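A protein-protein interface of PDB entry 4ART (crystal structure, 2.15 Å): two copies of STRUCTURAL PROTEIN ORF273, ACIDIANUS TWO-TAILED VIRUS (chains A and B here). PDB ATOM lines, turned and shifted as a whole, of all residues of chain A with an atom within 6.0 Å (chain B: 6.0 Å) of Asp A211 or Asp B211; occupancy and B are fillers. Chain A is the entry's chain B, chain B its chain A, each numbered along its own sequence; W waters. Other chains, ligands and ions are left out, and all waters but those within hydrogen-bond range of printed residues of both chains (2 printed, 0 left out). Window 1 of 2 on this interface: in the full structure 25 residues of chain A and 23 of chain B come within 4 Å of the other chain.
The backbone NH of Tyr B210 is in hydrogen-bond range of the backbone carbonyl oxygen of Ala B199.
O of Ala B199 sits at hydrogen-bond distance from N of Asp B211 (3.0 Å).
OG1 of Thr B209 is in hydrogen-bond range of OE1 of Glu B212 (2.8 Å).
N of Tyr A210 lies within hydrogen-bond range of O of Ala A199, 3.5 Å away.
N of Asp A211 lies within hydrogen-bond range of O of Ala A199 (3.0 Å).
OG1 of Thr A209 lies within hydrogen-bond range of OE1 of Glu A212.
Arg B215 touches Ile A113.
Ala A199 touches Glu B200 (O to OE1, 3.9 Å).
Ala A199 touches Arg B215.
Ala B199 touches Glu A200 (O to OE1, 3.8 Å).
Glu A200 touches Asp B211 (CD to CB, 3.5 Å).
Glu B212 touches Glu A200 (CG to OE2, 3.2 Å).
Arg B215 touches Tyr A210.
Glu B200 touches Asp A211 (OE1 to CB, 3.8 Å).
CG of Glu A212 touches OE2 of Glu B200, 3.1 Å away.
Ala B199 touches Arg A215.
The side-chain carboxylate (OE1) of Glu B200 sits at hydrogen-bond distance from the side-chain hydroxyl (OG1) of Thr A209, at 2.7 Å.
OG1 of Thr B209 lies within hydrogen-bond range of OE1 of Glu A200, at 2.6 Å.
OD2 of Asp A211 lies close to OD2 of Asp B211, at 2.4 Å.
The side-chain carboxylate of Asp B211 lies within salt-bridge range of the guanidinium group of Arg A215, at 2.8 Å.
The guanidinium group of Arg B215 is in salt-bridge range of the side-chain carboxylate of Asp A211 (2.6 Å).
O of Glu A200 lies close to OE1 of Glu B200 (3.4 Å).
Water W1 bridges OE2 of Glu A200 and NH1 of Arg B215.
Water W2 lies within hydrogen-bond range of the side-chain carboxylate of Glu B200 (2.8 Å) and the guanidinium group of Arg A215 (2.8 Å).
Of the printed residues of chain B, Ala A199 touches Glu B200 and Arg B215.
Printed residues of chain B within 4 Å of Glu A200: Ala B199 (3.8 Å), Glu B200 (3.4 Å), Thr B209 (2.6 Å), Asp B211 (3.5 Å) and Glu B212 (3.2 Å).
Printed residues of chain B within 4 Å of Asp A211: Glu B200, Asp B211 and Arg B215.
Leu A214 touches none of the printed residues of chain B.
Printed residues of chain B within 4 Å of Arg A215: Ala B199 and Asp B211.
Ile A216 touches none of the printed residues of chain B.
Printed residues of chain A within 4 Å of Glu B200: Ala A199, Glu A200, Thr A209, Asp A211 and Glu A212.
Asp B211 touches three residues of chain A.
The nearest residue of chain B that does not touch Asp A211 is Ala B199 (5.8 Å).
Of the 11 printed residues of chain B, 6 touch a printed residue of chain A.
Hydrophobic or aromatic side chains of chain B within 4 Å of the printed part of chain A: Ala B199.
Hydrophobic or aromatic side chains of chain A that line the printed part of chain B: Ile A113, Ala A199 and Tyr A210.
Among the printed residues, Asp or Glu carboxylates within 4 Å of a Lys or Arg side-chain nitrogen of the other chain: Asp A211 with Arg B215 (2.6 Å) and Arg A215 with Asp B211 (2.8 Å).
Ala A199 touches Glu B200, and with the chains exchanged Glu A200 touches Ala B199.
Ala A199 touches Arg B215, and with the chains exchanged Arg A215 touches Ala B199.
Glu A200 touches Asp B211, and with the chains exchanged Asp A211 touches Glu B200.
Tyr A210 touches Arg B215, but with the chains exchanged Arg A215 does not touch Tyr B210 (4.7 Å).
Positions printed for both chains: 113, 199, 200, 209, 210, 211, 212, 213, 214, 215 and 216.
Of the 16 pairs that touch across the chains among the printed residues, 14 have their exchanged pair printed and touching as well.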
ATOM      1  N   ILE A 113     -23.152  -7.758 -25.974  1.00  0.00           N
ATOM      2  CA  ILE A 113     -22.995  -8.230 -24.601  1.00  0.00           C
ATOM      3  C   ILE A 113     -24.269  -8.936 -24.107  1.00  0.00           C
ATOM      4  O   ILE A 113     -24.155  -9.859 -23.309  1.00  0.00           O
ATOM      5  CB  ILE A 113     -22.450  -7.159 -23.602  1.00  0.00           C
ATOM      6  CG1 ILE A 113     -21.846  -7.845 -22.343  1.00  0.00           C
ATOM      7  CG2 ILE A 113     -23.523  -6.111 -23.250  1.00  0.00           C
ATOM      8  CD1 ILE A 113     -20.789  -7.067 -21.537  1.00  0.00           C
ATOM      9  N   ALA A 199     -21.791  -4.498 -18.644  1.00  0.00           N
ATOM     10  CA  ALA A 199     -21.680  -3.533 -19.757  1.00  0.00           C
ATOM     11  C   ALA A 199     -21.276  -2.131 -19.360  1.00  0.00           C
ATOM     12  O   ALA A 199     -20.707  -1.415 -20.179  1.00  0.00           O
ATOM     13  CB  ALA A 199     -23.007  -3.455 -20.504  1.00  0.00           C
ATOM     14  N   GLU A 200     -21.660  -1.695 -18.153  1.00  0.00           N
ATOM     15  CA  GLU A 200     -21.480  -0.311 -17.682  1.00  0.00           C
ATOM     16  C   GLU A 200     -20.602  -0.117 -16.460  1.00  0.00           C
ATOM     17  O   GLU A 200     -20.263   1.022 -16.151  1.00  0.00           O
ATOM     18  CB  GLU A 200     -22.862   0.281 -17.359  1.00  0.00           C
ATOM     19  CG  GLU A 200     -23.834   0.280 -18.524  1.00  0.00           C
ATOM     20  CD  GLU A 200     -25.207   0.754 -18.106  1.00  0.00           C
ATOM     21  OE1 GLU A 200     -25.343   1.944 -17.745  1.00  0.00           O
ATOM     22  OE2 GLU A 200     -26.127  -0.096 -18.037  1.00  0.00           O
ATOM     23  N   THR A 209     -15.183   0.424 -19.783  1.00  0.00           N
ATOM     24  CA  THR A 209     -16.263  -0.541 -19.684  1.00  0.00           C
ATOM     25  C   THR A 209     -16.597  -1.069 -21.105  1.00  0.00           C
ATOM     26  O   THR A 209     -16.086  -0.538 -22.095  1.00  0.00           O
ATOM     27  CB  THR A 209     -17.494   0.137 -19.053  1.00  0.00           C
ATOM     28  OG1 THR A 209     -17.921   1.183 -19.897  1.00  0.00           O
ATOM     29  CG2 THR A 209     -17.224   0.689 -17.640  1.00  0.00           C
ATOM     30  N   TYR A 210     -17.446  -2.094 -21.204  1.00  0.00           N
ATOM     31  CA  TYR A 210     -17.871  -2.579 -22.509  1.00  0.00           C
ATOM     32  C   TYR A 210     -18.541  -1.440 -23.346  1.00  0.00           C
ATOM     33  O   TYR A 210     -18.243  -1.314 -24.540  1.00  0.00           O
ATOM     34  CB  TYR A 210     -18.789  -3.821 -22.337  1.00  0.00           C
ATOM     35  CG  TYR A 210     -19.510  -4.238 -23.601  1.00  0.00           C
ATOM     36  CD1 TYR A 210     -20.747  -3.690 -23.930  1.00  0.00           C
ATOM     37  CD2 TYR A 210     -18.936  -5.138 -24.494  1.00  0.00           C
ATOM     38  CE1 TYR A 210     -21.403  -4.035 -25.108  1.00  0.00           C
ATOM     39  CE2 TYR A 210     -19.607  -5.523 -25.662  1.00  0.00           C
ATOM     40  CZ  TYR A 210     -20.822  -4.937 -25.982  1.00  0.00           C
ATOM     41  OH  TYR A 210     -21.513  -5.262 -27.131  1.00  0.00           O
ATOM     42  N   ASP A 211     -19.424  -0.607 -22.722  1.00  0.00           N
ATOM     43  CA  ASP A 211     -20.147   0.455 -23.454  1.00  0.00           C
ATOM     44  C   ASP A 211     -19.210   1.561 -23.957  1.00  0.00           C
ATOM     45  O   ASP A 211     -19.374   2.025 -25.082  1.00  0.00           O
ATOM     46  CB  ASP A 211     -21.349   1.011 -22.656  1.00  0.00           C
ATOM     47  CG  ASP A 211     -22.552   0.087 -22.549  1.00  0.00           C
ATOM     48  OD1 ASP A 211     -22.511  -1.021 -23.121  1.00  0.00           O
ATOM     49  OD2 ASP A 211     -23.541   0.474 -21.894  1.00  0.00           O
ATOM     50  N   GLU A 212     -18.189   1.921 -23.172  1.00  0.00           N
ATOM     51  CA  GLU A 212     -17.180   2.886 -23.617  1.00  0.00           C
ATOM     52  C   GLU A 212     -16.332   2.258 -24.726  1.00  0.00           C
ATOM     53  O   GLU A 212     -15.964   2.934 -25.693  1.00  0.00           O
ATOM     54  CB  GLU A 212     -16.267   3.261 -22.464  1.00  0.00           C
ATOM     55  CG  GLU A 212     -16.969   4.047 -21.381  1.00  0.00           C
ATOM     56  CD  GLU A 212     -16.102   4.254 -20.169  1.00  0.00           C
ATOM     57  OE1 GLU A 212     -15.908   3.277 -19.424  1.00  0.00           O
ATOM     58  OE2 GLU A 212     -15.568   5.371 -19.990  1.00  0.00           O
ATOM     59  N   ALA A 213     -16.028   0.966 -24.600  1.00  0.00           N
ATOM     60  CA  ALA A 213     -15.212   0.283 -25.614  1.00  0.00           C
ATOM     61  C   ALA A 213     -15.979   0.083 -26.968  1.00  0.00           C
ATOM     62  O   ALA A 213     -15.358  -0.157 -28.001  1.00  0.00           O
ATOM     63  CB  ALA A 213     -14.630  -1.010 -25.060  1.00  0.00           C
ATOM     64  N   LEU A 214     -17.314   0.239 -26.975  1.00  0.00           N
ATOM     65  CA  LEU A 214     -18.088   0.244 -28.219  1.00  0.00           C
ATOM     66  C   LEU A 214     -17.993   1.662 -28.825  1.00  0.00           C
ATOM     67  O   LEU A 214     -17.712   1.814 -29.998  1.00  0.00           O
ATOM     68  CB  LEU A 214     -19.588  -0.053 -27.954  1.00  0.00           C
ATOM     69  CG  LEU A 214     -20.038  -1.492 -27.702  1.00  0.00           C
ATOM     70  CD1 LEU A 214     -21.546  -1.495 -27.296  1.00  0.00           C
ATOM     71  CD2 LEU A 214     -19.881  -2.343 -28.960  1.00  0.00           C
ATOM     72  N   ARG A 215     -18.229   2.687 -28.007  1.00  0.00           N
ATOM     73  CA  ARG A 215     -18.280   4.112 -28.380  1.00  0.00           C
ATOM     74  C   ARG A 215     -16.951   4.730 -28.868  1.00  0.00           C
ATOM     75  O   ARG A 215     -16.921   5.325 -29.940  1.00  0.00           O
ATOM     76  CB  ARG A 215     -18.879   4.948 -27.234  1.00  0.00           C
ATOM     77  CG  ARG A 215     -20.382   4.715 -27.015  1.00  0.00           C
ATOM     78  CD  ARG A 215     -20.962   5.676 -25.999  1.00  0.00           C
ATOM     79  NE  ARG A 215     -22.421   5.559 -25.912  1.00  0.00           N
ATOM     80  CZ  ARG A 215     -23.088   5.074 -24.870  1.00  0.00           C
ATOM     81  NH1 ARG A 215     -22.438   4.669 -23.784  1.00  0.00           N
ATOM     82  NH2 ARG A 215     -24.409   4.993 -24.902  1.00  0.00           N
ATOM     83  N   ILE A 216     -15.869   4.592 -28.076  1.00  0.00           N
ATOM     84  CA  ILE A 216     -14.543   5.162 -28.377  1.00  0.00           C
ATOM     85  C   ILE A 216     -13.848   4.656 -29.689  1.00  0.00           C
ATOM     86  O   ILE A 216     -13.542   5.503 -30.534  1.00  0.00           O
ATOM     87  CB  ILE A 216     -13.615   5.222 -27.127  1.00  0.00           C
ATOM     88  CG1 ILE A 216     -14.303   5.966 -25.952  1.00  0.00           C
ATOM     89  CG2 ILE A 216     -12.270   5.847 -27.468  1.00  0.00           C
ATOM     90  CD1 ILE A 216     -13.715   5.738 -24.535  1.00  0.00           C
ATOM     91  N   ILE B 113     -25.592   9.228 -27.767  1.00  0.00           N
ATOM     92  CA  ILE B 113     -25.165  10.075 -26.645  1.00  0.00           C
ATOM     93  C   ILE B 113     -23.982  10.927 -27.089  1.00  0.00           C
ATOM     94  O   ILE B 113     -23.964  12.142 -26.859  1.00  0.00           O
ATOM     95  CB  ILE B 113     -24.868   9.217 -25.363  1.00  0.00           C
ATOM     96  CG1 ILE B 113     -26.174   8.896 -24.632  1.00  0.00           C
ATOM     97  CG2 ILE B 113     -23.886   9.913 -24.370  1.00  0.00           C
ATOM     98  CD1 ILE B 113     -26.935  10.113 -23.967  1.00  0.00           C
ATOM     99  N   ALA B 199     -24.266   8.645 -19.689  1.00  0.00           N
ATOM    100  CA  ALA B 199     -24.816   7.398 -20.219  1.00  0.00           C
ATOM    101  C   ALA B 199     -24.841   6.196 -19.307  1.00  0.00           C
ATOM    102  O   ALA B 199     -25.694   5.326 -19.479  1.00  0.00           O
ATOM    103  CB  ALA B 199     -24.097   7.045 -21.495  1.00  0.00           C
ATOM    104  N   GLU B 200     -23.860   6.090 -18.409  1.00  0.00           N
ATOM    105  CA  GLU B 200     -23.635   4.892 -17.576  1.00  0.00           C
ATOM    106  C   GLU B 200     -23.698   5.083 -16.068  1.00  0.00           C
ATOM    107  O   GLU B 200     -23.615   4.089 -15.337  1.00  0.00           O
ATOM    108  CB  GLU B 200     -22.247   4.317 -17.896  1.00  0.00           C
ATOM    109  CG  GLU B 200     -22.007   3.983 -19.345  1.00  0.00           C
ATOM    110  CD  GLU B 200     -20.572   3.576 -19.575  1.00  0.00           C
ATOM    111  OE1 GLU B 200     -20.244   2.405 -19.297  1.00  0.00           O
ATOM    112  OE2 GLU B 200     -19.777   4.409 -20.052  1.00  0.00           O
ATOM    113  N   THR B 209     -29.968   3.928 -15.517  1.00  0.00           N
ATOM    114  CA  THR B 209     -28.962   4.686 -16.243  1.00  0.00           C
ATOM    115  C   THR B 209     -29.477   4.688 -17.688  1.00  0.00           C
ATOM    116  O   THR B 209     -30.334   3.857 -18.028  1.00  0.00           O
ATOM    117  CB  THR B 209     -27.609   4.025 -16.183  1.00  0.00           C
ATOM    118  OG1 THR B 209     -27.669   2.736 -16.791  1.00  0.00           O
ATOM    119  CG2 THR B 209     -27.026   3.967 -14.804  1.00  0.00           C
ATOM    120  N   TYR B 210     -28.961   5.599 -18.527  1.00  0.00           N
ATOM    121  CA  TYR B 210     -29.377   5.735 -19.930  1.00  0.00           C
ATOM    122  C   TYR B 210     -29.162   4.456 -20.736  1.00  0.00           C
ATOM    123  O   TYR B 210     -30.004   4.098 -21.562  1.00  0.00           O
ATOM    124  CB  TYR B 210     -28.607   6.897 -20.575  1.00  0.00           C
ATOM    125  CG  TYR B 210     -29.072   7.218 -21.979  1.00  0.00           C
ATOM    126  CD1 TYR B 210     -30.200   8.006 -22.200  1.00  0.00           C
ATOM    127  CD2 TYR B 210     -28.388   6.728 -23.088  1.00  0.00           C
ATOM    128  CE1 TYR B 210     -30.643   8.287 -23.495  1.00  0.00           C
ATOM    129  CE2 TYR B 210     -28.840   6.974 -24.381  1.00  0.00           C
ATOM    130  CZ  TYR B 210     -29.946   7.780 -24.579  1.00  0.00           C
ATOM    131  OH  TYR B 210     -30.346   8.052 -25.853  1.00  0.00           O
ATOM    132  N   ASP B 211     -28.008   3.798 -20.545  1.00  0.00           N
ATOM    133  CA  ASP B 211     -27.702   2.586 -21.302  1.00  0.00           C
ATOM    134  C   ASP B 211     -28.667   1.445 -20.978  1.00  0.00           C
ATOM    135  O   ASP B 211     -29.077   0.724 -21.882  1.00  0.00           O
ATOM    136  CB  ASP B 211     -26.207   2.204 -21.158  1.00  0.00           C
ATOM    137  CG  ASP B 211     -25.256   3.102 -21.959  1.00  0.00           C
ATOM    138  OD1 ASP B 211     -25.741   4.040 -22.617  1.00  0.00           O
ATOM    139  OD2 ASP B 211     -24.007   2.874 -21.902  1.00  0.00           O
ATOM    140  N   GLU B 212     -29.093   1.321 -19.706  1.00  0.00           N
ATOM    141  CA  GLU B 212     -30.125   0.334 -19.326  1.00  0.00           C
ATOM    142  C   GLU B 212     -31.466   0.722 -19.960  1.00  0.00           C
ATOM    143  O   GLU B 212     -32.225  -0.152 -20.382  1.00  0.00           O
ATOM    144  CB  GLU B 212     -30.346   0.372 -17.820  1.00  0.00           C
ATOM    145  CG  GLU B 212     -29.201  -0.216 -17.052  1.00  0.00           C
ATOM    146  CD  GLU B 212     -29.389  -0.035 -15.573  1.00  0.00           C
ATOM    147  OE1 GLU B 212     -29.222   1.105 -15.075  1.00  0.00           O
ATOM    148  OE2 GLU B 212     -29.782  -1.028 -14.925  1.00  0.00           O
ATOM    149  N   ALA B 213     -31.759   2.038 -20.015  1.00  0.00           N
ATOM    150  CA  ALA B 213     -33.011   2.544 -20.595  1.00  0.00           C
ATOM    151  C   ALA B 213     -33.102   2.315 -22.112  1.00  0.00           C
ATOM    152  O   ALA B 213     -34.195   2.298 -22.664  1.00  0.00           O
ATOM    153  CB  ALA B 213     -33.190   4.022 -20.259  1.00  0.00           C
ATOM    154  N   LEU B 214     -31.973   2.110 -22.787  1.00  0.00           N
ATOM    155  CA  LEU B 214     -31.988   1.784 -24.210  1.00  0.00           C
ATOM    156  C   LEU B 214     -32.264   0.275 -24.315  1.00  0.00           C
ATOM    157  O   LEU B 214     -33.097  -0.142 -25.100  1.00  0.00           O
ATOM    158  CB  LEU B 214     -30.602   2.061 -24.854  1.00  0.00           C
ATOM    159  CG  LEU B 214     -30.169   3.501 -25.174  1.00  0.00           C
ATOM    160  CD1 LEU B 214     -28.722   3.510 -25.656  1.00  0.00           C
ATOM    161  CD2 LEU B 214     -31.068   4.141 -26.235  1.00  0.00           C
ATOM    162  N   ARG B 215     -31.520  -0.543 -23.546  1.00  0.00           N
ATOM    163  CA  ARG B 215     -31.555  -2.020 -23.538  1.00  0.00           C
ATOM    164  C   ARG B 215     -32.870  -2.677 -23.141  1.00  0.00           C
ATOM    165  O   ARG B 215     -33.347  -3.535 -23.868  1.00  0.00           O
ATOM    166  CB  ARG B 215     -30.378  -2.573 -22.735  1.00  0.00           C
ATOM    167  CG  ARG B 215     -29.030  -2.374 -23.452  1.00  0.00           C
ATOM    168  CD  ARG B 215     -27.901  -3.109 -22.751  1.00  0.00           C
ATOM    169  NE  ARG B 215     -26.665  -3.084 -23.549  1.00  0.00           N
ATOM    170  CZ  ARG B 215     -25.613  -2.316 -23.293  1.00  0.00           C
ATOM    171  NH1 ARG B 215     -25.607  -1.520 -22.232  1.00  0.00           N
ATOM    172  NH2 ARG B 215     -24.535  -2.382 -24.061  1.00  0.00           N
ATOM    173  N   ILE B 216     -33.465  -2.276 -22.013  1.00  0.00           N
ATOM    174  CA  ILE B 216     -34.727  -2.859 -21.539  1.00  0.00           C
ATOM    175  C   ILE B 216     -35.901  -2.805 -22.567  1.00  0.00           C
ATOM    176  O   ILE B 216     -36.484  -3.855 -22.839  1.00  0.00           O
ATOM    177  CB  ILE B 216     -35.083  -2.363 -20.122  1.00  0.00           C
ATOM    178  CG1 ILE B 216     -34.048  -2.903 -19.100  1.00  0.00           C
ATOM    179  CG2 ILE B 216     -36.515  -2.733 -19.762  1.00  0.00           C
ATOM    180  CD1 ILE B 216     -34.122  -2.241 -17.765  1.00  0.00           C
HETATM  181  O   HOH W   1     -26.995  -2.018 -19.716  1.00  0.00           O
HETATM  182  O   HOH W   2     -20.082   5.655 -22.541  1.00  0.00           O
